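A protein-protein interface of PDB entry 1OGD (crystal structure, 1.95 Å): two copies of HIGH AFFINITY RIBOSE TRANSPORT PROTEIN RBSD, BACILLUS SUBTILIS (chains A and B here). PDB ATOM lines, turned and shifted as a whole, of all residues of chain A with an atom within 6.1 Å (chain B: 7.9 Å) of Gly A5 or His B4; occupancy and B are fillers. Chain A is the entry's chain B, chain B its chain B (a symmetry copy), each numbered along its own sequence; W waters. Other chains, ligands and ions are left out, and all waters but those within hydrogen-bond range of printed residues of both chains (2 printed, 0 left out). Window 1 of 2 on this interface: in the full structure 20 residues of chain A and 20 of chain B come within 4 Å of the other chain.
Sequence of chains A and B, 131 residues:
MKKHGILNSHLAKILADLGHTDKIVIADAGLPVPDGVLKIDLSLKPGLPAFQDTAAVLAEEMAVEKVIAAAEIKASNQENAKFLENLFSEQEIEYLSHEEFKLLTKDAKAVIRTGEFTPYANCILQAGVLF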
ATOM      1  N   LYS A   2      18.125  19.385  -6.432  1.00  0.00           N
ATOM      2  CA  LYS A   2      17.587  20.534  -5.718  1.00  0.00           C
ATOM      3  C   LYS A   2      17.288  20.082  -4.289  1.00  0.00           C
ATOM      4  O   LYS A   2      16.565  19.110  -4.079  1.00  0.00           O
ATOM      5  CB  LYS A   2      16.308  21.007  -6.424  1.00  0.00           C
ATOM      6  CG  LYS A   2      15.647  22.239  -5.839  1.00  0.00           C
ATOM      7  CD  LYS A   2      14.602  22.811  -6.804  1.00  0.00           C
ATOM      8  CE  LYS A   2      13.399  21.895  -6.975  1.00  0.00           C
ATOM      9  NZ  LYS A   2      12.470  21.974  -5.819  1.00  0.00           N
ATOM     10  N   LYS A   3      17.854  20.783  -3.311  1.00  0.00           N
ATOM     11  CA  LYS A   3      17.655  20.429  -1.906  1.00  0.00           C
ATOM     12  C   LYS A   3      16.285  20.757  -1.332  1.00  0.00           C
ATOM     13  O   LYS A   3      15.713  19.959  -0.593  1.00  0.00           O
ATOM     14  CB  LYS A   3      18.697  21.124  -1.023  1.00  0.00           C
ATOM     15  CG  LYS A   3      20.110  20.601  -1.137  1.00  0.00           C
ATOM     16  CD  LYS A   3      21.005  21.374  -0.187  1.00  0.00           C
ATOM     17  CE  LYS A   3      22.436  20.884  -0.235  1.00  0.00           C
ATOM     18  NZ  LYS A   3      23.285  21.645   0.728  1.00  0.00           N
ATOM     19  N   HIS A   4      15.756  21.927  -1.667  1.00  0.00           N
ATOM     20  CA  HIS A   4      14.481  22.352  -1.104  1.00  0.00           C
ATOM     21  C   HIS A   4      13.351  22.565  -2.095  1.00  0.00           C
ATOM     22  O   HIS A   4      13.559  22.599  -3.310  1.00  0.00           O
ATOM     23  CB  HIS A   4      14.701  23.639  -0.316  1.00  0.00           C
ATOM     24  CG  HIS A   4      15.855  23.565   0.634  1.00  0.00           C
ATOM     25  ND1 HIS A   4      16.824  24.544   0.706  1.00  0.00           N
ATOM     26  CD2 HIS A   4      16.204  22.620   1.536  1.00  0.00           C
ATOM     27  CE1 HIS A   4      17.723  24.201   1.613  1.00  0.00           C
ATOM     28  NE2 HIS A   4      17.370  23.038   2.130  1.00  0.00           N
ATOM     29  N   GLY A   5      12.148  22.714  -1.551  1.00  0.00           N
ATOM     30  CA  GLY A   5      10.983  22.957  -2.379  1.00  0.00           C
ATOM     31  C   GLY A   5      10.262  21.708  -2.836  1.00  0.00           C
ATOM     32  O   GLY A   5      10.603  20.595  -2.447  1.00  0.00           O
ATOM     33  N   ILE A   6       9.261  21.911  -3.679  1.00  0.00           N
ATOM     34  CA  ILE A   6       8.450  20.828  -4.208  1.00  0.00           C
ATOM     35  C   ILE A   6       9.323  19.921  -5.082  1.00  0.00           C
ATOM     36  O   ILE A   6      10.228  20.397  -5.776  1.00  0.00           O
ATOM     37  CB  ILE A   6       7.264  21.426  -4.991  1.00  0.00           C
ATOM     38  CG1 ILE A   6       6.164  20.382  -5.158  1.00  0.00           C
ATOM     39  CG2 ILE A   6       7.747  21.980  -6.329  1.00  0.00           C
ATOM     40  CD1 ILE A   6       4.823  20.998  -5.507  1.00  0.00           C
ATOM     41  N   LEU A   7       9.058  18.615  -5.033  1.00  0.00           N
ATOM     42  CA  LEU A   7       9.843  17.632  -5.777  1.00  0.00           C
ATOM     43  C   LEU A   7       9.593  17.588  -7.279  1.00  0.00           C
ATOM     44  O   LEU A   7      10.519  17.377  -8.057  1.00  0.00           O
ATOM     45  CB  LEU A   7       9.612  16.227  -5.204  1.00  0.00           C
ATOM     46  CG  LEU A   7      10.402  15.077  -5.840  1.00  0.00           C
ATOM     47  CD1 LEU A   7      11.892  15.317  -5.658  1.00  0.00           C
ATOM     48  CD2 LEU A   7       9.988  13.751  -5.207  1.00  0.00           C
ATOM     49  N   GLU A  60       1.797  23.242   1.351  1.00  0.00           N
ATOM     50  CA  GLU A  60       3.050  23.327   2.084  1.00  0.00           C
ATOM     51  C   GLU A  60       4.167  24.032   1.300  1.00  0.00           C
ATOM     52  O   GLU A  60       5.130  24.515   1.889  1.00  0.00           O
ATOM     53  CB  GLU A  60       3.492  21.911   2.476  1.00  0.00           C
ATOM     54  CG  GLU A  60       4.299  21.830   3.771  1.00  0.00           C
ATOM     55  CD  GLU A  60       5.740  22.285   3.607  1.00  0.00           C
ATOM     56  OE1 GLU A  60       6.389  22.594   4.634  1.00  0.00           O
ATOM     57  OE2 GLU A  60       6.230  22.320   2.454  1.00  0.00           O
ATOM     58  N   GLU A  61       4.029  24.113  -0.021  1.00  0.00           N
ATOM     59  CA  GLU A  61       5.071  24.728  -0.849  1.00  0.00           C
ATOM     60  C   GLU A  61       4.719  26.086  -1.455  1.00  0.00           C
ATOM     61  O   GLU A  61       5.577  26.756  -2.033  1.00  0.00           O
ATOM     62  CB  GLU A  61       5.445  23.772  -1.983  1.00  0.00           C
ATOM     63  CG  GLU A  61       5.967  22.417  -1.532  1.00  0.00           C
ATOM     64  CD  GLU A  61       7.253  22.517  -0.736  1.00  0.00           C
ATOM     65  OE1 GLU A  61       7.934  23.563  -0.809  1.00  0.00           O
ATOM     66  OE2 GLU A  61       7.589  21.539  -0.043  1.00  0.00           O
ATOM     67  N   MET B   1       3.003  32.851  -3.806  1.00  0.00           N
ATOM     68  CA  MET B   1       4.479  32.760  -3.980  1.00  0.00           C
ATOM     69  C   MET B   1       5.024  31.428  -3.485  1.00  0.00           C
ATOM     70  O   MET B   1       4.418  30.766  -2.652  1.00  0.00           O
ATOM     71  CB  MET B   1       5.177  33.893  -3.227  1.00  0.00           C
ATOM     72  CG  MET B   1       4.991  35.270  -3.843  1.00  0.00           C
ATOM     73  SD  MET B   1       5.990  36.524  -3.005  1.00  0.00           S
ATOM     74  CE  MET B   1       7.622  36.151  -3.632  1.00  0.00           C
ATOM     75  N   LYS B   2       6.182  31.051  -4.011  1.00  0.00           N
ATOM     76  CA  LYS B   2       6.849  29.811  -3.645  1.00  0.00           C
ATOM     77  C   LYS B   2       7.483  30.024  -2.271  1.00  0.00           C
ATOM     78  O   LYS B   2       8.255  30.962  -2.078  1.00  0.00           O
ATOM     79  CB  LYS B   2       7.917  29.487  -4.700  1.00  0.00           C
ATOM     80  CG  LYS B   2       8.672  28.188  -4.499  1.00  0.00           C
ATOM     81  CD  LYS B   2       9.451  27.806  -5.764  1.00  0.00           C
ATOM     82  CE  LYS B   2      10.598  28.762  -6.056  1.00  0.00           C
ATOM     83  NZ  LYS B   2      11.770  28.510  -5.180  1.00  0.00           N
ATOM     84  N   LYS B   3       7.149  29.159  -1.318  1.00  0.00           N
ATOM     85  CA  LYS B   3       7.678  29.278   0.039  1.00  0.00           C
ATOM     86  C   LYS B   3       9.137  28.886   0.214  1.00  0.00           C
ATOM     87  O   LYS B   3       9.882  29.561   0.921  1.00  0.00           O
ATOM     88  CB  LYS B   3       6.858  28.425   1.014  1.00  0.00           C
ATOM     89  CG  LYS B   3       5.468  28.931   1.322  1.00  0.00           C
ATOM     90  CD  LYS B   3       4.805  27.993   2.313  1.00  0.00           C
ATOM     91  CE  LYS B   3       3.412  28.456   2.684  1.00  0.00           C
ATOM     92  NZ  LYS B   3       2.797  27.528   3.678  1.00  0.00           N
ATOM     93  N   HIS B   4       9.550  27.799  -0.425  1.00  0.00           N
ATOM     94  CA  HIS B   4      10.912  27.312  -0.256  1.00  0.00           C
ATOM     95  C   HIS B   4      11.774  27.289  -1.505  1.00  0.00           C
ATOM     96  O   HIS B   4      11.287  27.454  -2.625  1.00  0.00           O
ATOM     97  CB  HIS B   4      10.858  25.907   0.337  1.00  0.00           C
ATOM     98  CG  HIS B   4       9.960  25.799   1.528  1.00  0.00           C
ATOM     99  ND1 HIS B   4       9.015  24.803   1.662  1.00  0.00           N
ATOM    100  CD2 HIS B   4       9.850  26.574   2.632  1.00  0.00           C
ATOM    101  CE1 HIS B   4       8.360  24.972   2.798  1.00  0.00           C
ATOM    102  NE2 HIS B   4       8.847  26.039   3.404  1.00  0.00           N
ATOM    103  N   GLY B   5      13.068  27.076  -1.290  1.00  0.00           N
ATOM    104  CA  GLY B   5      14.002  26.997  -2.396  1.00  0.00           C
ATOM    105  C   GLY B   5      14.620  28.319  -2.795  1.00  0.00           C
ATOM    106  O   GLY B   5      14.403  29.345  -2.157  1.00  0.00           O
ATOM    107  N   ILE B   6      15.392  28.279  -3.871  1.00  0.00           N
ATOM    108  CA  ILE B   6      16.078  29.451  -4.387  1.00  0.00           C
ATOM    109  C   ILE B   6      15.043  30.473  -4.868  1.00  0.00           C
ATOM    110  O   ILE B   6      13.992  30.102  -5.401  1.00  0.00           O
ATOM    111  CB  ILE B   6      17.036  29.016  -5.513  1.00  0.00           C
ATOM    112  CG1 ILE B   6      18.087  30.095  -5.757  1.00  0.00           C
ATOM    113  CG2 ILE B   6      16.242  28.683  -6.775  1.00  0.00           C
ATOM    114  CD1 ILE B   6      19.297  29.572  -6.508  1.00  0.00           C
ATOM    115  N   LEU B   7      15.338  31.758  -4.666  1.00  0.00           N
ATOM    116  CA  LEU B   7      14.421  32.835  -5.031  1.00  0.00           C
ATOM    117  C   LEU B   7      14.313  33.134  -6.520  1.00  0.00           C
ATOM    118  O   LEU B   7      13.234  33.454  -7.014  1.00  0.00           O
ATOM    119  CB  LEU B   7      14.807  34.130  -4.302  1.00  0.00           C
ATOM    120  CG  LEU B   7      13.913  35.354  -4.535  1.00  0.00           C
ATOM    121  CD1 LEU B   7      12.502  35.057  -4.051  1.00  0.00           C
ATOM    122  CD2 LEU B   7      14.490  36.563  -3.805  1.00  0.00           C
ATOM    123  N   ALA B  12      15.555  28.431 -10.305  1.00  0.00           N
ATOM    124  CA  ALA B  12      14.696  27.419  -9.690  1.00  0.00           C
ATOM    125  C   ALA B  12      14.313  26.383 -10.743  1.00  0.00           C
ATOM    126  O   ALA B  12      14.232  25.192 -10.453  1.00  0.00           O
ATOM    127  CB  ALA B  12      13.437  28.066  -9.112  1.00  0.00           C
ATOM    128  N   GLU B  61      21.290  25.603  -1.958  1.00  0.00           N
ATOM    129  CA  GLU B  61      20.071  25.114  -2.609  1.00  0.00           C
ATOM    130  C   GLU B  61      20.244  23.883  -3.499  1.00  0.00           C
ATOM    131  O   GLU B  61      19.262  23.302  -3.963  1.00  0.00           O
ATOM    132  CB  GLU B  61      19.462  26.238  -3.449  1.00  0.00           C
ATOM    133  CG  GLU B  61      19.087  27.488  -2.669  1.00  0.00           C
ATOM    134  CD  GLU B  61      18.021  27.231  -1.622  1.00  0.00           C
ATOM    135  OE1 GLU B  61      17.321  26.199  -1.707  1.00  0.00           O
ATOM    136  OE2 GLU B  61      17.876  28.074  -0.717  1.00  0.00           O
HETATM  137  O   HOH W   1      16.787  23.990  -3.289  1.00  0.00           O
HETATM  138  O   HOH W   2       8.127  26.015  -2.082  1.00  0.00           O
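Hydrophobic or aromatic side chains of chain A within 4 Å of the printed part of chain B: His A4. Of the 9 printed residues of chain B, 5 touch a printed residue of chain A. Printed residues of chain B that touch a printed residue of chain A: Lys B2, Lys B3, His B4, Gly B5 and Glu B61. Hydrophobic or aromatic side chains of chain B within 4 Å of the printed part of chain A: His B4. Along chain B the printed residues that touch a printed residue of chain A span positions 2 to 61. Among the printed residues, no Asp or Glu carboxylate lies within 4 Å of a Lys or Arg side-chain nitrogen of the other chain.
Water W1 lies within hydrogen-bond range of the backbone carbonyl oxygen of Glu B61, the backbone NH of His A4 and the backbone NH of Lys A3. Water W2 lies within hydrogen-bond range of O of Glu A61 (2.7 Å), N of His B4 (2.8 Å) and N of Lys B3 (3.4 Å).
Glu B61 touches Lys A2. Gly B5 touches His A4 (N to CB, 3.9 Å). Gly A5 touches His B4 (N to CB, 3.9 Å). O of Glu A60 touches CD of Lys B3 (3.5 Å). Glu A60 touches His B4 (O to CE1, 3.4 Å). Lys B2 touches Glu A61.
N of Lys A3 sits at hydrogen-bond distance from O of Glu B61 (3.0 Å). A ring nitrogen (ND1) of His A4 lies within hydrogen-bond range of the side-chain carboxylate of Glu B61, 3.0 Å away. The backbone carbonyl oxygen (O) of Glu A61 sits at hydrogen-bond distance from the backbone NH (N) of Lys B3. OE1 of Glu A61 sits at hydrogen-bond distance from ND1 of His B4, at 3.0 Å.
Of chain A, only Gly A5 (3.9 Å), Glu A60 (3.4 Å) and Glu A61 (3.0 Å) come within 4 Å of His B4. Of the printed residues of chain B, Glu A60 touches Lys B3 (3.5 Å) and His B4 (3.4 Å). Of the printed residues of chain B, Lys A3 touches Glu B61 (3.0 Å). Printed residues of chain A within 4 Å of Gly B5: His A4 (3.9 Å). Of the printed residues of chain A, Glu B61 touches Lys A2, Lys A3 and His A4. Ile A6 touches none of the printed residues of chain B. The nearest residue of chain A that does not touch His B4 is His A4 (4.5 Å).
Lys A2 touches Glu B61, and with the chains exchanged Glu A61 touches Lys B2. Lys A3 touches Glu B61, and with the chains exchanged Glu A61 touches Lys B3. His A4 touches Gly B5, and with the chains exchanged Gly A5 touches His B4. His A4 touches Glu B61, and with the chains exchanged Glu A61 touches His B4. 7 positions are printed for both chains.
The backbone carbonyl oxygen of His A4 sits at hydrogen-bond distance from the side-chain amino group of Lys A2 (2.8 Å). The backbone carbonyl oxygen of Ile A6 sits at hydrogen-bond distance from the side-chain amino group of Lys A2. The backbone carbonyl oxygen (O) of His B4 lies within hydrogen-bond range of the side-chain amino group (NZ) of Lys B2 (2.8 Å). O of Ile B6 lies within hydrogen-bond range of NZ of Lys B2.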
